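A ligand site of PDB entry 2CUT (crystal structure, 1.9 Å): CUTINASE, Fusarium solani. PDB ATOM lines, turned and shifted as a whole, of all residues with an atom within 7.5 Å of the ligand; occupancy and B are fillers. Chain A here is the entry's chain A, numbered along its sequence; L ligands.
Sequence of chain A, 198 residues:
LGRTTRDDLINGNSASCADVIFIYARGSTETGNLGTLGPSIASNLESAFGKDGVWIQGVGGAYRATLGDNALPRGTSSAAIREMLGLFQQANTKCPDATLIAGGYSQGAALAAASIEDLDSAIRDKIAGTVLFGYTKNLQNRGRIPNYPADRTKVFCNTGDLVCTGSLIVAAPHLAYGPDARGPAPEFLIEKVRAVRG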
ATOM      1  N   ARG A  26     -27.290  19.273  13.645  1.00  0.00           N
ATOM      2  CA  ARG A  26     -26.742  18.998  14.970  1.00  0.00           C
ATOM      3  C   ARG A  26     -26.460  17.510  15.209  1.00  0.00           C
ATOM      4  O   ARG A  26     -26.775  16.652  14.411  1.00  0.00           O
ATOM      5  CB  ARG A  26     -27.728  19.537  16.026  1.00  0.00           C
ATOM      6  CG  ARG A  26     -28.977  18.663  16.210  1.00  0.00           C
ATOM      7  CD  ARG A  26     -30.022  19.363  17.029  1.00  0.00           C
ATOM      8  NE  ARG A  26     -31.109  18.424  17.238  1.00  0.00           N
ATOM      9  CZ  ARG A  26     -32.041  18.104  16.296  1.00  0.00           C
ATOM     10  NH1 ARG A  26     -32.107  18.615  15.063  1.00  0.00           N
ATOM     11  NH2 ARG A  26     -32.997  17.213  16.609  1.00  0.00           N
ATOM     12  N   GLY A  27     -25.751  17.187  16.304  1.00  0.00           N
ATOM     13  CA  GLY A  27     -25.441  15.816  16.666  1.00  0.00           C
ATOM     14  C   GLY A  27     -26.637  15.114  17.348  1.00  0.00           C
ATOM     15  O   GLY A  27     -27.638  15.737  17.713  1.00  0.00           O
ATOM     16  N   SER A  28     -26.539  13.802  17.526  1.00  0.00           N
ATOM     17  CA  SER A  28     -27.568  13.004  18.175  1.00  0.00           C
ATOM     18  C   SER A  28     -27.778  13.553  19.586  1.00  0.00           C
ATOM     19  O   SER A  28     -26.786  13.953  20.262  1.00  0.00           O
ATOM     20  CB  SER A  28     -27.131  11.551  18.280  1.00  0.00           C
ATOM     21  OG  SER A  28     -26.818  10.976  17.022  1.00  0.00           O
ATOM     22  N   THR A  29     -29.066  13.666  19.909  1.00  0.00           N
ATOM     23  CA  THR A  29     -29.503  14.094  21.209  1.00  0.00           C
ATOM     24  C   THR A  29     -29.322  15.575  21.502  1.00  0.00           C
ATOM     25  O   THR A  29     -29.732  16.034  22.580  1.00  0.00           O
ATOM     26  CB  THR A  29     -28.729  13.108  22.167  1.00  0.00           C
ATOM     27  OG1 THR A  29     -29.665  12.027  22.321  1.00  0.00           O
ATOM     28  CG2 THR A  29     -28.092  13.746  23.367  1.00  0.00           C
ATOM     29  N   GLU A  30     -28.782  16.378  20.585  1.00  0.00           N
ATOM     30  CA  GLU A  30     -28.604  17.779  20.883  1.00  0.00           C
ATOM     31  C   GLU A  30     -29.904  18.579  20.876  1.00  0.00           C
ATOM     32  O   GLU A  30     -30.859  18.161  20.218  1.00  0.00           O
ATOM     33  CB  GLU A  30     -27.630  18.308  19.895  1.00  0.00           C
ATOM     34  CG  GLU A  30     -26.236  17.751  20.079  1.00  0.00           C
ATOM     35  CD  GLU A  30     -25.240  18.765  19.583  1.00  0.00           C
ATOM     36  OE1 GLU A  30     -25.264  19.151  18.420  1.00  0.00           O
ATOM     37  OE2 GLU A  30     -24.421  19.180  20.368  1.00  0.00           O
ATOM     38  N   THR A  36     -24.994  22.272  20.377  1.00  0.00           N
ATOM     39  CA  THR A  36     -23.942  22.948  21.115  1.00  0.00           C
ATOM     40  C   THR A  36     -23.001  23.774  20.247  1.00  0.00           C
ATOM     41  O   THR A  36     -22.564  24.843  20.679  1.00  0.00           O
ATOM     42  CB  THR A  36     -23.097  21.941  21.909  1.00  0.00           C
ATOM     43  OG1 THR A  36     -22.490  20.999  21.029  1.00  0.00           O
ATOM     44  CG2 THR A  36     -23.977  21.198  22.916  1.00  0.00           C
ATOM     45  N   TYR A  63     -35.668  15.533  11.167  1.00  0.00           N
ATOM     46  CA  TYR A  63     -34.390  15.106  11.673  1.00  0.00           C
ATOM     47  C   TYR A  63     -34.503  15.188  13.178  1.00  0.00           C
ATOM     48  O   TYR A  63     -34.390  16.228  13.817  1.00  0.00           O
ATOM     49  CB  TYR A  63     -33.241  15.991  11.207  1.00  0.00           C
ATOM     50  CG  TYR A  63     -31.911  15.606  11.795  1.00  0.00           C
ATOM     51  CD1 TYR A  63     -31.514  14.277  11.858  1.00  0.00           C
ATOM     52  CD2 TYR A  63     -31.091  16.608  12.267  1.00  0.00           C
ATOM     53  CE1 TYR A  63     -30.304  13.959  12.402  1.00  0.00           C
ATOM     54  CE2 TYR A  63     -29.866  16.307  12.803  1.00  0.00           C
ATOM     55  CZ  TYR A  63     -29.489  14.977  12.876  1.00  0.00           C
ATOM     56  OH  TYR A  63     -28.287  14.646  13.491  1.00  0.00           O
ATOM     57  N   ALA A  65     -32.443  13.383  15.167  1.00  0.00           N
ATOM     58  CA  ALA A  65     -31.123  13.201  15.755  1.00  0.00           C
ATOM     59  C   ALA A  65     -31.146  12.104  16.854  1.00  0.00           C
ATOM     60  O   ALA A  65     -30.636  12.227  17.956  1.00  0.00           O
ATOM     61  CB  ALA A  65     -30.637  14.549  16.349  1.00  0.00           C
ATOM     62  N   THR A  66     -31.706  10.963  16.467  1.00  0.00           N
ATOM     63  CA  THR A  66     -31.900   9.758  17.251  1.00  0.00           C
ATOM     64  C   THR A  66     -30.577   9.033  17.251  1.00  0.00           C
ATOM     65  O   THR A  66     -29.930   8.827  16.202  1.00  0.00           O
ATOM     66  CB  THR A  66     -33.013   9.012  16.531  1.00  0.00           C
ATOM     67  OG1 THR A  66     -34.189   9.592  17.060  1.00  0.00           O
ATOM     68  CG2 THR A  66     -32.971   7.504  16.643  1.00  0.00           C
ATOM     69  N   LEU A  67     -30.136   8.599  18.423  1.00  0.00           N
ATOM     70  CA  LEU A  67     -28.859   7.894  18.535  1.00  0.00           C
ATOM     71  C   LEU A  67     -28.911   6.591  17.746  1.00  0.00           C
ATOM     72  O   LEU A  67     -27.949   6.256  17.062  1.00  0.00           O
ATOM     73  CB  LEU A  67     -28.633   7.716  20.021  1.00  0.00           C
ATOM     74  CG  LEU A  67     -27.310   7.688  20.693  1.00  0.00           C
ATOM     75  CD1 LEU A  67     -26.264   8.672  20.163  1.00  0.00           C
ATOM     76  CD2 LEU A  67     -27.669   8.054  22.118  1.00  0.00           C
ATOM     77  N   ASN A  70     -27.738   6.372  13.799  1.00  0.00           N
ATOM     78  CA  ASN A  70     -26.332   6.333  13.489  1.00  0.00           C
ATOM     79  C   ASN A  70     -25.950   5.007  12.894  1.00  0.00           C
ATOM     80  O   ASN A  70     -25.019   4.911  12.114  1.00  0.00           O
ATOM     81  CB  ASN A  70     -25.473   6.525  14.703  1.00  0.00           C
ATOM     82  CG  ASN A  70     -25.405   7.951  15.189  1.00  0.00           C
ATOM     83  OD1 ASN A  70     -24.864   8.847  14.510  1.00  0.00           O
ATOM     84  ND2 ASN A  70     -25.893   8.247  16.389  1.00  0.00           N
ATOM     85  N   GLY A  75     -25.606   6.508   7.928  1.00  0.00           N
ATOM     86  CA  GLY A  75     -25.274   7.129   9.178  1.00  0.00           C
ATOM     87  C   GLY A  75     -26.400   7.983   9.676  1.00  0.00           C
ATOM     88  O   GLY A  75     -26.178   8.691  10.633  1.00  0.00           O
ATOM     89  N   TYR A 105     -22.479  18.181  12.888  1.00  0.00           N
ATOM     90  CA  TYR A 105     -21.704  17.512  13.922  1.00  0.00           C
ATOM     91  C   TYR A 105     -22.266  16.101  14.107  1.00  0.00           C
ATOM     92  O   TYR A 105     -23.479  15.860  14.176  1.00  0.00           O
ATOM     93  CB  TYR A 105     -21.807  18.355  15.192  1.00  0.00           C
ATOM     94  CG  TYR A 105     -21.275  17.730  16.491  1.00  0.00           C
ATOM     95  CD1 TYR A 105     -20.066  17.061  16.553  1.00  0.00           C
ATOM     96  CD2 TYR A 105     -22.074  17.797  17.612  1.00  0.00           C
ATOM     97  CE1 TYR A 105     -19.656  16.459  17.722  1.00  0.00           C
ATOM     98  CE2 TYR A 105     -21.675  17.191  18.789  1.00  0.00           C
ATOM     99  CZ  TYR A 105     -20.477  16.526  18.825  1.00  0.00           C
ATOM    100  OH  TYR A 105     -20.113  15.916  19.991  1.00  0.00           O
ATOM    101  N   SER A 106     -21.328  15.153  14.106  1.00  0.00           N
ATOM    102  CA  SER A 106     -21.577  13.755  14.427  1.00  0.00           C
ATOM    103  C   SER A 106     -22.626  13.198  13.466  1.00  0.00           C
ATOM    104  O   SER A 106     -22.335  13.184  12.266  1.00  0.00           O
ATOM    105  CB  SER A 106     -21.980  13.756  15.907  1.00  0.00           C
ATOM    106  OG  SER A 106     -21.900  12.454  16.477  1.00  0.00           O
ATOM    107  N   GLN A 107     -23.822  12.749  13.902  1.00  0.00           N
ATOM    108  CA  GLN A 107     -24.813  12.277  12.954  1.00  0.00           C
ATOM    109  C   GLN A 107     -25.200  13.374  11.957  1.00  0.00           C
ATOM    110  O   GLN A 107     -25.512  13.057  10.802  1.00  0.00           O
ATOM    111  CB  GLN A 107     -26.084  11.827  13.688  1.00  0.00           C
ATOM    112  CG  GLN A 107     -27.131  11.314  12.715  1.00  0.00           C
ATOM    113  CD  GLN A 107     -28.451  10.799  13.273  1.00  0.00           C
ATOM    114  OE1 GLN A 107     -29.392  10.525  12.519  1.00  0.00           O
ATOM    115  NE2 GLN A 107     -28.582  10.681  14.589  1.00  0.00           N
ATOM    116  N   GLY A 108     -25.242  14.634  12.369  1.00  0.00           N
ATOM    117  CA  GLY A 108     -25.513  15.768  11.476  1.00  0.00           C
ATOM    118  C   GLY A 108     -24.415  15.941  10.400  1.00  0.00           C
ATOM    119  O   GLY A 108     -24.703  16.379   9.263  1.00  0.00           O
ATOM    120  N   ALA A 109     -23.160  15.544  10.702  1.00  0.00           N
ATOM    121  CA  ALA A 109     -22.096  15.543   9.715  1.00  0.00           C
ATOM    122  C   ALA A 109     -22.335  14.425   8.702  1.00  0.00           C
ATOM    123  O   ALA A 109     -22.118  14.612   7.502  1.00  0.00           O
ATOM    124  CB  ALA A 109     -20.751  15.345  10.393  1.00  0.00           C
ATOM    125  N   PHE A 133     -17.878  18.222  11.823  1.00  0.00           N
ATOM    126  CA  PHE A 133     -17.174  17.995  13.099  1.00  0.00           C
ATOM    127  C   PHE A 133     -17.536  16.593  13.551  1.00  0.00           C
ATOM    128  O   PHE A 133     -18.724  16.234  13.506  1.00  0.00           O
ATOM    129  CB  PHE A 133     -17.638  18.906  14.235  1.00  0.00           C
ATOM    130  CG  PHE A 133     -17.693  20.383  13.889  1.00  0.00           C
ATOM    131  CD1 PHE A 133     -18.815  20.882  13.244  1.00  0.00           C
ATOM    132  CD2 PHE A 133     -16.640  21.188  14.254  1.00  0.00           C
ATOM    133  CE1 PHE A 133     -18.911  22.216  12.932  1.00  0.00           C
ATOM    134  CE2 PHE A 133     -16.743  22.532  13.936  1.00  0.00           C
ATOM    135  CZ  PHE A 133     -17.873  23.040  13.299  1.00  0.00           C
ATOM    136  N   GLY A 134     -16.538  15.816  14.020  1.00  0.00           N
ATOM    137  CA  GLY A 134     -16.721  14.470  14.521  1.00  0.00           C
ATOM    138  C   GLY A 134     -17.514  13.709  13.493  1.00  0.00           C
ATOM    139  O   GLY A 134     -18.548  13.173  13.833  1.00  0.00           O
ATOM    140  N   THR A 136     -18.933  11.062  11.418  1.00  0.00           N
ATOM    141  CA  THR A 136     -19.091   9.621  11.629  1.00  0.00           C
ATOM    142  C   THR A 136     -18.700   8.763  10.446  1.00  0.00           C
ATOM    143  O   THR A 136     -18.500   7.553  10.589  1.00  0.00           O
ATOM    144  CB  THR A 136     -20.542   9.289  12.000  1.00  0.00           C
ATOM    145  OG1 THR A 136     -21.391   9.928  11.051  1.00  0.00           O
ATOM    146  CG2 THR A 136     -20.878   9.773  13.406  1.00  0.00           C
ATOM    147  N   ASP A 161     -11.055  11.002  18.899  1.00  0.00           N
ATOM    148  CA  ASP A 161     -12.467  10.899  18.664  1.00  0.00           C
ATOM    149  C   ASP A 161     -12.647   9.652  17.790  1.00  0.00           C
ATOM    150  O   ASP A 161     -12.515   9.643  16.562  1.00  0.00           O
ATOM    151  CB  ASP A 161     -12.940  12.160  17.972  1.00  0.00           C
ATOM    152  CG  ASP A 161     -14.442  12.122  17.698  1.00  0.00           C
ATOM    153  OD1 ASP A 161     -15.109  11.119  17.986  1.00  0.00           O
ATOM    154  OD2 ASP A 161     -14.974  13.119  17.215  1.00  0.00           O
ATOM    155  N   VAL A 163     -15.262   8.151  16.592  1.00  0.00           N
ATOM    156  CA  VAL A 163     -16.255   8.132  15.497  1.00  0.00           C
ATOM    157  C   VAL A 163     -15.639   8.479  14.123  1.00  0.00           C
ATOM    158  O   VAL A 163     -16.171   8.126  13.087  1.00  0.00           O
ATOM    159  CB  VAL A 163     -17.469   9.119  15.766  1.00  0.00           C
ATOM    160  CG1 VAL A 163     -17.988   8.801  17.174  1.00  0.00           C
ATOM    161  CG2 VAL A 163     -17.107  10.593  15.502  1.00  0.00           C
ATOM    162  N   SER A 167     -15.861   3.848  14.252  1.00  0.00           N
ATOM    163  CA  SER A 167     -16.742   3.253  15.222  1.00  0.00           C
ATOM    164  C   SER A 167     -17.743   4.298  15.651  1.00  0.00           C
ATOM    165  O   SER A 167     -17.753   5.430  15.139  1.00  0.00           O
ATOM    166  CB  SER A 167     -15.930   2.749  16.429  1.00  0.00           C
ATOM    167  OG  SER A 167     -15.448   3.748  17.301  1.00  0.00           O
ATOM    168  N   LEU A 168     -18.598   3.903  16.583  1.00  0.00           N
ATOM    169  CA  LEU A 168     -19.600   4.770  17.120  1.00  0.00           C
ATOM    170  C   LEU A 168     -19.334   4.928  18.608  1.00  0.00           C
ATOM    171  O   LEU A 168     -20.176   5.426  19.351  1.00  0.00           O
ATOM    172  CB  LEU A 168     -20.953   4.147  16.776  1.00  0.00           C
ATOM    173  CG  LEU A 168     -21.385   4.336  15.302  1.00  0.00           C
ATOM    174  CD1 LEU A 168     -22.783   3.762  15.070  1.00  0.00           C
ATOM    175  CD2 LEU A 168     -21.478   5.825  14.960  1.00  0.00           C
ATOM    176  N   ILE A 169     -18.122   4.573  19.072  1.00  0.00           N
ATOM    177  CA  ILE A 169     -17.847   4.788  20.476  1.00  0.00           C
ATOM    178  C   ILE A 169     -17.628   6.280  20.702  1.00  0.00           C
ATOM    179  O   ILE A 169     -16.801   6.911  20.015  1.00  0.00           O
ATOM    180  CB  ILE A 169     -16.585   4.070  20.986  1.00  0.00           C
ATOM    181  CG1 ILE A 169     -16.661   2.586  20.697  1.00  0.00           C
ATOM    182  CG2 ILE A 169     -16.458   4.315  22.490  1.00  0.00           C
ATOM    183  CD1 ILE A 169     -17.962   2.006  21.223  1.00  0.00           C
ATOM    184  N   VAL A 170     -18.321   6.841  21.682  1.00  0.00           N
ATOM    185  CA  VAL A 170     -18.103   8.199  22.088  1.00  0.00           C
ATOM    186  C   VAL A 170     -17.056   8.326  23.189  1.00  0.00           C
ATOM    187  O   VAL A 170     -17.176   7.829  24.312  1.00  0.00           O
ATOM    188  CB  VAL A 170     -19.403   8.840  22.552  1.00  0.00           C
ATOM    189  CG1 VAL A 170     -19.162  10.303  22.867  1.00  0.00           C
ATOM    190  CG2 VAL A 170     -20.450   8.750  21.445  1.00  0.00           C
ATOM    191  N   HIS A 174     -14.613  13.612  21.250  1.00  0.00           N
ATOM    192  CA  HIS A 174     -15.810  13.846  20.468  1.00  0.00           C
ATOM    193  C   HIS A 174     -16.604  15.019  20.996  1.00  0.00           C
ATOM    194  O   HIS A 174     -17.362  15.614  20.236  1.00  0.00           O
ATOM    195  CB  HIS A 174     -16.743  12.624  20.467  1.00  0.00           C
ATOM    196  CG  HIS A 174     -17.860  12.733  19.417  1.00  0.00           C
ATOM    197  ND1 HIS A 174     -17.740  12.854  18.088  1.00  0.00           N
ATOM    198  CD2 HIS A 174     -19.210  12.658  19.696  1.00  0.00           C
ATOM    199  CE1 HIS A 174     -18.935  12.842  17.559  1.00  0.00           C
ATOM    200  NE2 HIS A 174     -19.806  12.725  18.524  1.00  0.00           N
ATOM    201  N   LEU A 175     -16.412  15.313  22.275  1.00  0.00           N
ATOM    202  CA  LEU A 175     -17.093  16.361  22.945  1.00  0.00           C
ATOM    203  C   LEU A 175     -16.206  17.597  22.965  1.00  0.00           C
ATOM    204  O   LEU A 175     -16.480  18.549  23.679  1.00  0.00           O
ATOM    205  CB  LEU A 175     -17.441  15.902  24.389  1.00  0.00           C
ATOM    206  CG  LEU A 175     -18.522  14.826  24.749  1.00  0.00           C
ATOM    207  CD1 LEU A 175     -19.704  14.931  23.797  1.00  0.00           C
ATOM    208  CD2 LEU A 175     -18.009  13.419  24.543  1.00  0.00           C
HETATM  209  C1  LIG L   1     -21.911   9.486  17.962  1.00  0.00           C
HETATM  210  C2  LIG L   1     -22.057   8.001  17.715  1.00  0.00           C
HETATM  211  C3  LIG L   1     -23.368  13.655  19.230  1.00  0.00           C
HETATM  212  C4  LIG L   1     -22.590  13.827  20.535  1.00  0.00           C
HETATM  213  O1  LIG L   1     -22.967  10.187  17.261  1.00  0.00           O
HETATM  214  O2  LIG L   1     -22.995  12.352  18.785  1.00  0.00           O
HETATM  215  O3  LIG L   1     -24.417  12.112  16.635  1.00  0.00           O
HETATM  216  P1  LIG L   1     -23.130  11.806  17.278  1.00  0.00           P
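OG of Ser 106 is covalently linked to P1 of the ligand (1.6 Å). N of Ser 28 lies within hydrogen-bond range of O3 of the ligand (2.9 Å). The side-chain hydroxyl (OG) of Ser 28 is in hydrogen-bond range of an oxygen (O3) of the ligand (2.7 Å). The backbone NH of Gln 107 sits at hydrogen-bond distance from an oxygen (O3) of the ligand (2.9 Å). A ring nitrogen (NE2) of His 174 sits at hydrogen-bond distance from an oxygen (O2) of the ligand, at 3.2 Å.
The side-chain hydroxyl of Ser 106 is in hydrogen-bond range of a ring nitrogen (NE2) of His 174. The backbone NH (N) of Ser 106 lies within hydrogen-bond range of the backbone carbonyl oxygen (O) of Phe 133 (2.9 Å). The side-chain hydroxyl (OG) of Ser 28 is in hydrogen-bond range of the side-chain amide nitrogen (NE2) of Gln 107, 3.0 Å away. The side-chain amide nitrogen of Asn 70 sits at hydrogen-bond distance from the side-chain hydroxyl of Ser 28. The backbone carbonyl oxygen of His 174 is in hydrogen-bond range of the side-chain hydroxyl of Tyr 105 (2.8 Å). ND1 of His 174 sits at hydrogen-bond distance from OD2 of Asp 161, 2.9 Å away. The backbone carbonyl oxygen (O) of Tyr 105 sits close to the backbone NH (N) of Gly 27. OE1 of Glu 30 lies within hydrogen-bond range of N of Gly 27 (2.9 Å).
Residues that only touch the ligand: Tyr 105 (3.3 Å), Leu 168 (3.6 Å), Asn 70 (3.6 Å), Gly 27 (3.8 Å) and Val 170 (3.8 Å). Hydrophobic or aromatic side chains that line the ligand: Tyr 105, Leu 168, Val 170 and His 174. Nine residues have an atom within 4 Å of the ligand: Gly 27, Ser 28, Asn 70, Tyr 105, Ser 106, Gln 107, Leu 168, Val 170 and His 174. The nearest printed residue that does not touch the ligand is Val 163 (4.1 Å).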
